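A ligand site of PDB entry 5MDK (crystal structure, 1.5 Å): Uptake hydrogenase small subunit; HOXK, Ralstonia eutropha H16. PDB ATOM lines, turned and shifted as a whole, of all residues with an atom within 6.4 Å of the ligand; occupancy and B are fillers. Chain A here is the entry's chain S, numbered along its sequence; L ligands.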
ATOM      1  N   ILE A 186      21.603  15.808 -31.130  1.00  0.00           N
ATOM      2  CA  ILE A 186      21.272  16.536 -29.897  1.00  0.00           C
ATOM      3  C   ILE A 186      19.921  17.237 -30.046  1.00  0.00           C
ATOM      4  O   ILE A 186      19.083  17.196 -29.161  1.00  0.00           O
ATOM      5  CB  ILE A 186      22.351  17.592 -29.563  1.00  0.00           C
ATOM      6  CG1 ILE A 186      23.758  16.998 -29.442  1.00  0.00           C
ATOM      7  CG2 ILE A 186      22.021  18.339 -28.273  1.00  0.00           C
ATOM      8  CD1 ILE A 186      23.880  15.852 -28.480  1.00  0.00           C
ATOM      9  N   HIS A 187      19.743  17.888 -31.202  1.00  0.00           N
ATOM     10  CA  HIS A 187      18.562  18.689 -31.543  1.00  0.00           C
ATOM     11  C   HIS A 187      17.235  17.897 -31.546  1.00  0.00           C
ATOM     12  O   HIS A 187      16.172  18.487 -31.366  1.00  0.00           O
ATOM     13  CB  HIS A 187      18.857  19.327 -32.910  1.00  0.00           C
ATOM     14  CG  HIS A 187      17.855  20.322 -33.400  1.00  0.00           C
ATOM     15  ND1 HIS A 187      17.740  21.577 -32.868  1.00  0.00           N
ATOM     16  CD2 HIS A 187      16.979  20.262 -34.428  1.00  0.00           C
ATOM     17  CE1 HIS A 187      16.803  22.248 -33.518  1.00  0.00           C
ATOM     18  NE2 HIS A 187      16.329  21.465 -34.477  1.00  0.00           N
ATOM     19  N   ASP A 188      17.286  16.564 -31.734  1.00  0.00           N
ATOM     20  CA  ASP A 188      16.062  15.758 -31.808  1.00  0.00           C
ATOM     21  C   ASP A 188      15.216  15.878 -30.525  1.00  0.00           C
ATOM     22  O   ASP A 188      14.025  16.167 -30.603  1.00  0.00           O
ATOM     23  CB  ASP A 188      16.383  14.257 -32.059  1.00  0.00           C
ATOM     24  CG  ASP A 188      16.978  13.979 -33.458  1.00  0.00           C
ATOM     25  OD1 ASP A 188      16.830  14.831 -34.353  1.00  0.00           O
ATOM     26  OD2 ASP A 188      17.589  12.899 -33.678  1.00  0.00           O
ATOM     27  N   CYS A 190      16.440  17.702 -27.564  1.00  0.00           N
ATOM     28  CA  CYS A 190      16.821  18.831 -26.757  1.00  0.00           C
ATOM     29  C   CYS A 190      15.594  19.491 -26.151  1.00  0.00           C
ATOM     30  O   CYS A 190      14.653  19.820 -26.881  1.00  0.00           O
ATOM     31  CB  CYS A 190      17.564  19.856 -27.605  1.00  0.00           C
ATOM     32  SG  CYS A 190      18.066  21.331 -26.692  1.00  0.00           S
ATOM     33  N   TYR A 191      15.609  19.711 -24.837  1.00  0.00           N
ATOM     34  CA  TYR A 191      14.458  20.311 -24.147  1.00  0.00           C
ATOM     35  C   TYR A 191      14.165  21.747 -24.611  1.00  0.00           C
ATOM     36  O   TYR A 191      13.078  22.252 -24.347  1.00  0.00           O
ATOM     37  CB  TYR A 191      14.608  20.274 -22.611  1.00  0.00           C
ATOM     38  CG  TYR A 191      15.464  21.392 -22.077  1.00  0.00           C
ATOM     39  CD1 TYR A 191      16.852  21.343 -22.189  1.00  0.00           C
ATOM     40  CD2 TYR A 191      14.907  22.509 -21.461  1.00  0.00           C
ATOM     41  CE1 TYR A 191      17.639  22.378 -21.722  1.00  0.00           C
ATOM     42  CE2 TYR A 191      15.684  23.547 -20.993  1.00  0.00           C
ATOM     43  CZ  TYR A 191      17.060  23.462 -21.123  1.00  0.00           C
ATOM     44  OH  TYR A 191      17.857  24.468 -20.683  1.00  0.00           O
ATOM     45  N   ARG A 192      15.115  22.409 -25.277  1.00  0.00           N
ATOM     46  CA  ARG A 192      14.882  23.752 -25.827  1.00  0.00           C
ATOM     47  C   ARG A 192      14.248  23.749 -27.235  1.00  0.00           C
ATOM     48  O   ARG A 192      13.975  24.816 -27.786  1.00  0.00           O
ATOM     49  CB  ARG A 192      16.174  24.580 -25.845  1.00  0.00           C
ATOM     50  CG  ARG A 192      16.752  24.770 -24.442  1.00  0.00           C
ATOM     51  CD  ARG A 192      17.805  25.856 -24.408  1.00  0.00           C
ATOM     52  NE  ARG A 192      18.420  25.976 -23.075  1.00  0.00           N
ATOM     53  CZ  ARG A 192      19.006  27.077 -22.603  1.00  0.00           C
ATOM     54  NH1 ARG A 192      19.108  28.183 -23.329  1.00  0.00           N
ATOM     55  NH2 ARG A 192      19.515  27.038 -21.374  1.00  0.00           N
ATOM     56  N   ARG A 193      14.007  22.567 -27.784  1.00  0.00           N
ATOM     57  CA  ARG A 193      13.466  22.419 -29.138  1.00  0.00           C
ATOM     58  C   ARG A 193      12.138  23.161 -29.361  1.00  0.00           C
ATOM     59  O   ARG A 193      11.961  23.767 -30.404  1.00  0.00           O
ATOM     60  CB  ARG A 193      13.373  20.935 -29.518  1.00  0.00           C
ATOM     61  CG  ARG A 193      12.807  20.620 -30.898  1.00  0.00           C
ATOM     62  CD  ARG A 193      13.713  21.106 -32.013  1.00  0.00           C
ATOM     63  NE  ARG A 193      13.160  20.773 -33.327  1.00  0.00           N
ATOM     64  CZ  ARG A 193      13.377  19.647 -33.999  1.00  0.00           C
ATOM     65  NH1 ARG A 193      14.158  18.684 -33.511  1.00  0.00           N
ATOM     66  NH2 ARG A 193      12.786  19.478 -35.190  1.00  0.00           N
ATOM     67  N   PRO A 194      11.208  23.125 -28.377  1.00  0.00           N
ATOM     68  CA  PRO A 194       9.977  23.905 -28.556  1.00  0.00           C
ATOM     69  C   PRO A 194      10.254  25.393 -28.780  1.00  0.00           C
ATOM     70  O   PRO A 194       9.535  26.025 -29.533  1.00  0.00           O
ATOM     71  CB  PRO A 194       9.218  23.665 -27.248  1.00  0.00           C
ATOM     72  CG  PRO A 194       9.663  22.309 -26.813  1.00  0.00           C
ATOM     73  CD  PRO A 194      11.127  22.263 -27.186  1.00  0.00           C
ATOM     74  N   HIS A 195      11.312  25.927 -28.165  1.00  0.00           N
ATOM     75  CA  HIS A 195      11.691  27.314 -28.449  1.00  0.00           C
ATOM     76  C   HIS A 195      12.217  27.466 -29.879  1.00  0.00           C
ATOM     77  O   HIS A 195      11.847  28.425 -30.584  1.00  0.00           O
ATOM     78  CB  HIS A 195      12.719  27.844 -27.433  1.00  0.00           C
ATOM     79  CG  HIS A 195      12.161  27.989 -26.055  1.00  0.00           C
ATOM     80  ND1 HIS A 195      11.061  28.760 -25.780  1.00  0.00           N
ATOM     81  CD2 HIS A 195      12.545  27.443 -24.875  1.00  0.00           C
ATOM     82  CE1 HIS A 195      10.806  28.709 -24.484  1.00  0.00           C
ATOM     83  NE2 HIS A 195      11.691  27.912 -23.922  1.00  0.00           N
ATOM     84  N   PHE A 196      13.063  26.548 -30.319  1.00  0.00           N
ATOM     85  CA  PHE A 196      13.561  26.569 -31.696  1.00  0.00           C
ATOM     86  C   PHE A 196      12.384  26.570 -32.664  1.00  0.00           C
ATOM     87  O   PHE A 196      12.335  27.383 -33.604  1.00  0.00           O
ATOM     88  CB  PHE A 196      14.413  25.329 -31.985  1.00  0.00           C
ATOM     89  CG  PHE A 196      14.860  25.215 -33.411  1.00  0.00           C
ATOM     90  CD1 PHE A 196      14.102  24.530 -34.354  1.00  0.00           C
ATOM     91  CD2 PHE A 196      16.063  25.780 -33.813  1.00  0.00           C
ATOM     92  CE1 PHE A 196      14.528  24.407 -35.658  1.00  0.00           C
ATOM     93  CE2 PHE A 196      16.496  25.647 -35.130  1.00  0.00           C
ATOM     94  CZ  PHE A 196      15.719  24.963 -36.051  1.00  0.00           C
ATOM     95  N   PHE A 201      14.822  32.585 -29.657  1.00  0.00           N
ATOM     96  CA  PHE A 201      16.277  32.449 -29.608  1.00  0.00           C
ATOM     97  C   PHE A 201      16.968  33.446 -28.692  1.00  0.00           C
ATOM     98  O   PHE A 201      16.573  34.609 -28.598  1.00  0.00           O
ATOM     99  CB  PHE A 201      16.856  32.634 -31.012  1.00  0.00           C
ATOM    100  CG  PHE A 201      16.330  31.677 -32.030  1.00  0.00           C
ATOM    101  CD1 PHE A 201      16.744  30.353 -32.049  1.00  0.00           C
ATOM    102  CD2 PHE A 201      15.407  32.092 -32.987  1.00  0.00           C
ATOM    103  CE1 PHE A 201      16.252  29.455 -32.992  1.00  0.00           C
ATOM    104  CE2 PHE A 201      14.920  31.215 -33.936  1.00  0.00           C
ATOM    105  CZ  PHE A 201      15.337  29.899 -33.943  1.00  0.00           C
ATOM    106  N   PHE A 214      15.752  30.072 -23.801  1.00  0.00           N
ATOM    107  CA  PHE A 214      15.437  30.027 -25.234  1.00  0.00           C
ATOM    108  C   PHE A 214      16.543  29.288 -26.006  1.00  0.00           C
ATOM    109  O   PHE A 214      17.669  29.096 -25.511  1.00  0.00           O
ATOM    110  CB  PHE A 214      15.244  31.445 -25.791  1.00  0.00           C
ATOM    111  CG  PHE A 214      13.853  32.030 -25.554  1.00  0.00           C
ATOM    112  CD1 PHE A 214      12.960  31.477 -24.630  1.00  0.00           C
ATOM    113  CD2 PHE A 214      13.476  33.159 -26.250  1.00  0.00           C
ATOM    114  CE1 PHE A 214      11.711  32.034 -24.448  1.00  0.00           C
ATOM    115  CE2 PHE A 214      12.221  33.726 -26.055  1.00  0.00           C
ATOM    116  CZ  PHE A 214      11.341  33.153 -25.157  1.00  0.00           C
ATOM    117  N   CYS A 215      16.213  28.847 -27.212  1.00  0.00           N
ATOM    118  CA  CYS A 215      17.125  28.067 -28.034  1.00  0.00           C
ATOM    119  C   CYS A 215      18.442  28.814 -28.298  1.00  0.00           C
ATOM    120  O   CYS A 215      18.478  30.057 -28.443  1.00  0.00           O
ATOM    121  CB  CYS A 215      16.431  27.665 -29.336  1.00  0.00           C
ATOM    122  SG  CYS A 215      17.513  26.966 -30.601  1.00  0.00           S
ATOM    123  N   LEU A 216      19.537  28.053 -28.365  1.00  0.00           N
ATOM    124  CA  LEU A 216      20.898  28.604 -28.521  1.00  0.00           C
ATOM    125  C   LEU A 216      21.435  28.563 -29.956  1.00  0.00           C
ATOM    126  O   LEU A 216      22.618  28.850 -30.175  1.00  0.00           O
ATOM    127  CB  LEU A 216      21.861  27.874 -27.588  1.00  0.00           C
ATOM    128  CG  LEU A 216      21.543  28.098 -26.102  1.00  0.00           C
ATOM    129  CD1 LEU A 216      22.228  27.098 -25.176  1.00  0.00           C
ATOM    130  CD2 LEU A 216      21.930  29.505 -25.703  1.00  0.00           C
ATOM    131  N   TYR A 217      20.587  28.227 -30.926  1.00  0.00           N
ATOM    132  CA  TYR A 217      21.003  28.154 -32.351  1.00  0.00           C
ATOM    133  C   TYR A 217      21.740  29.399 -32.830  1.00  0.00           C
ATOM    134  O   TYR A 217      22.777  29.315 -33.498  1.00  0.00           O
ATOM    135  CB  TYR A 217      19.775  27.919 -33.238  1.00  0.00           C
ATOM    136  CG  TYR A 217      20.067  27.668 -34.709  1.00  0.00           C
ATOM    137  CD1 TYR A 217      20.169  28.727 -35.609  1.00  0.00           C
ATOM    138  CD2 TYR A 217      20.212  26.383 -35.188  1.00  0.00           C
ATOM    139  CE1 TYR A 217      20.407  28.496 -36.959  1.00  0.00           C
ATOM    140  CE2 TYR A 217      20.445  26.132 -36.532  1.00  0.00           C
ATOM    141  CZ  TYR A 217      20.551  27.195 -37.412  1.00  0.00           C
ATOM    142  OH  TYR A 217      20.792  26.972 -38.750  1.00  0.00           O
ATOM    143  N   LYS A 218      21.206  30.576 -32.520  1.00  0.00           N
ATOM    144  CA  LYS A 218      21.829  31.817 -32.983  1.00  0.00           C
ATOM    145  C   LYS A 218      23.125  32.212 -32.238  1.00  0.00           C
ATOM    146  O   LYS A 218      23.845  33.106 -32.694  1.00  0.00           O
ATOM    147  CB  LYS A 218      20.805  32.952 -32.967  1.00  0.00           C
ATOM    148  CG  LYS A 218      19.657  32.701 -33.933  1.00  0.00           C
ATOM    149  CD  LYS A 218      18.695  33.888 -34.042  1.00  0.00           C
ATOM    150  CE  LYS A 218      17.718  33.644 -35.169  1.00  0.00           C
ATOM    151  NZ  LYS A 218      16.741  34.772 -35.280  1.00  0.00           N
ATOM    152  N   CYS A 221      24.952  27.080 -31.514  1.00  0.00           N
ATOM    153  CA  CYS A 221      24.697  25.689 -31.135  1.00  0.00           C
ATOM    154  C   CYS A 221      24.781  24.758 -32.331  1.00  0.00           C
ATOM    155  O   CYS A 221      24.106  24.944 -33.333  1.00  0.00           O
ATOM    156  CB  CYS A 221      23.342  25.540 -30.444  1.00  0.00           C
ATOM    157  SG  CYS A 221      23.040  23.869 -29.839  1.00  0.00           S
ATOM    158  N   LYS A 222      25.622  23.740 -32.209  1.00  0.00           N
ATOM    159  CA  LYS A 222      25.789  22.743 -33.260  1.00  0.00           C
ATOM    160  C   LYS A 222      24.993  21.474 -32.979  1.00  0.00           C
ATOM    161  O   LYS A 222      25.174  20.455 -33.656  1.00  0.00           O
ATOM    162  CB  LYS A 222      27.281  22.449 -33.455  1.00  0.00           C
ATOM    163  CG  LYS A 222      28.106  23.681 -33.848  1.00  0.00           C
ATOM    164  CD  LYS A 222      27.452  24.483 -34.976  1.00  0.00           C
ATOM    165  CE  LYS A 222      28.330  25.590 -35.544  1.00  0.00           C
ATOM    166  NZ  LYS A 222      28.870  26.521 -34.523  1.00  0.00           N
ATOM    167  N   GLY A 223      24.053  21.534 -32.034  1.00  0.00           N
ATOM    168  CA  GLY A 223      23.171  20.421 -31.775  1.00  0.00           C
ATOM    169  C   GLY A 223      22.469  19.833 -32.996  1.00  0.00           C
ATOM    170  O   GLY A 223      22.309  18.615 -33.095  1.00  0.00           O
ATOM    171  N   PRO A 224      22.048  20.702 -33.955  1.00  0.00           N
ATOM    172  CA  PRO A 224      21.382  20.160 -35.137  1.00  0.00           C
ATOM    173  C   PRO A 224      22.213  19.265 -36.054  1.00  0.00           C
ATOM    174  O   PRO A 224      21.640  18.567 -36.885  1.00  0.00           O
ATOM    175  CB  PRO A 224      20.938  21.416 -35.892  1.00  0.00           C
ATOM    176  CG  PRO A 224      20.804  22.457 -34.843  1.00  0.00           C
ATOM    177  CD  PRO A 224      21.924  22.166 -33.887  1.00  0.00           C
ATOM    178  N   SER A 231      21.304  15.069 -24.853  1.00  0.00           N
ATOM    179  CA  SER A 231      19.989  15.643 -24.561  1.00  0.00           C
ATOM    180  C   SER A 231      19.103  14.716 -23.734  1.00  0.00           C
ATOM    181  O   SER A 231      18.162  15.180 -23.086  1.00  0.00           O
ATOM    182  CB  SER A 231      19.246  15.977 -25.865  1.00  0.00           C
ATOM    183  OG  SER A 231      19.909  16.993 -26.567  1.00  0.00           O
ATOM    184  N   PHE A 241      23.531  19.195 -19.230  1.00  0.00           N
ATOM    185  CA  PHE A 241      24.330  19.061 -20.432  1.00  0.00           C
ATOM    186  C   PHE A 241      24.640  20.468 -20.913  1.00  0.00           C
ATOM    187  O   PHE A 241      24.109  21.431 -20.355  1.00  0.00           O
ATOM    188  CB  PHE A 241      23.693  18.131 -21.479  1.00  0.00           C
ATOM    189  CG  PHE A 241      22.486  18.670 -22.198  1.00  0.00           C
ATOM    190  CD1 PHE A 241      21.306  18.919 -21.515  1.00  0.00           C
ATOM    191  CD2 PHE A 241      22.491  18.801 -23.586  1.00  0.00           C
ATOM    192  CE1 PHE A 241      20.171  19.354 -22.190  1.00  0.00           C
ATOM    193  CE2 PHE A 241      21.372  19.224 -24.274  1.00  0.00           C
ATOM    194  CZ  PHE A 241      20.203  19.508 -23.574  1.00  0.00           C
ATOM    195  N   ILE A 243      23.842  22.546 -23.228  1.00  0.00           N
ATOM    196  CA  ILE A 243      22.710  23.416 -23.566  1.00  0.00           C
ATOM    197  C   ILE A 243      21.890  23.770 -22.322  1.00  0.00           C
ATOM    198  O   ILE A 243      21.501  24.928 -22.158  1.00  0.00           O
ATOM    199  CB  ILE A 243      21.860  22.773 -24.679  1.00  0.00           C
ATOM    200  CG1 ILE A 243      22.649  22.845 -25.987  1.00  0.00           C
ATOM    201  CG2 ILE A 243      20.478  23.423 -24.798  1.00  0.00           C
ATOM    202  CD1 ILE A 243      22.405  21.713 -26.956  1.00  0.00           C
ATOM    203  N   GLY A 248      25.818  26.679 -26.204  1.00  0.00           N
ATOM    204  CA  GLY A 248      25.494  25.828 -27.340  1.00  0.00           C
ATOM    205  C   GLY A 248      26.423  24.619 -27.380  1.00  0.00           C
ATOM    206  O   GLY A 248      27.565  24.666 -26.933  1.00  0.00           O
ATOM    207  N   CYS A 249      25.915  23.516 -27.897  1.00  0.00           N
ATOM    208  CA  CYS A 249      26.766  22.398 -28.302  1.00  0.00           C
ATOM    209  C   CYS A 249      27.847  22.968 -29.252  1.00  0.00           C
ATOM    210  O   CYS A 249      27.546  23.784 -30.127  1.00  0.00           O
ATOM    211  CB  CYS A 249      25.910  21.361 -29.013  1.00  0.00           C
ATOM    212  SG  CYS A 249      26.777  19.951 -29.712  1.00  0.00           S
HETATM  213 FE1  LIG L   1      20.716  23.669 -29.902  1.00  0.00          FE
HETATM  214 FE2  LIG L   1      18.300  24.919 -29.974  1.00  0.00          FE
HETATM  215 FE3  LIG L   1      18.598  22.638 -28.513  1.00  0.00          FE
HETATM  216 FE4  LIG L   1      18.619  22.582 -31.209  1.00  0.00          FE
HETATM  217  S1  LIG L   1      16.855  23.177 -29.852  1.00  0.00           S
HETATM  218  S2  LIG L   1      20.082  21.487 -29.882  1.00  0.00           S
HETATM  219  S3  LIG L   1      19.720  24.502 -31.755  1.00  0.00           S
HETATM  220  S4  LIG L   1      19.610  24.702 -28.137  1.00  0.00           S
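ND1 of His 187 binds FE4 of the ligand. An iron atom (FE2) of the ligand is bound by the side-chain sulfur (SG) of Cys 215 (2.3 Å). An iron atom (FE3) of the ligand is bound by the side-chain sulfur (SG) of Cys 190 (2.3 Å). An iron atom (FE1) of the ligand is bound by the side-chain sulfur (SG) of Cys 221. The backbone NH (N) of Leu 216 sits close to a sulfur (S4) of the ligand (3.4 Å). The backbone NH (N) of Arg 193 lies close to a sulfur (S1) of the ligand (3.6 Å).
Merely in contact with the ligand: Arg 192 (3.7 Å), Phe 196 (3.9 Å), Tyr 217 (3.7 Å), Gly 223 (3.8 Å), Pro 224 (3.9 Å) and Ile 243 (3.7 Å). Hydrophobic or aromatic side chains that line the ligand: His 187, Phe 196, Leu 216, Tyr 217, Pro 224 and Ile 243. Within 4 Å of the ligand: His 187, Cys 190, Arg 192, Arg 193, Phe 196, Cys 215, Leu 216, Tyr 217, Cys 221, Gly 223, Pro 224 and Ile 243.
The backbone carbonyl oxygen (O) of His 187 sits at hydrogen-bond distance from the guanidinium group (NH1) of Arg 193 (2.9 Å). The backbone NH (N) of Tyr 217 lies close to the side-chain sulfur (SG) of Cys 215 (3.3 Å). The side-chain sulfur (SG) of Cys 190 lies close to the backbone NH (N) of Arg 192 (3.4 Å). O of Leu 216 is in hydrogen-bond range of N of Cys 221 (3.2 Å). The backbone NH (N) of Cys 249 lies close to the side-chain sulfur (SG) of Cys 221. O of Ile 243 sits at hydrogen-bond distance from NH2 of Arg 192. NH1 of Arg 192 is in hydrogen-bond range of O of Phe 214, 2.8 Å away. O of Gly 223 is in hydrogen-bond range of N of Ile 186, at 3.5 Å.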
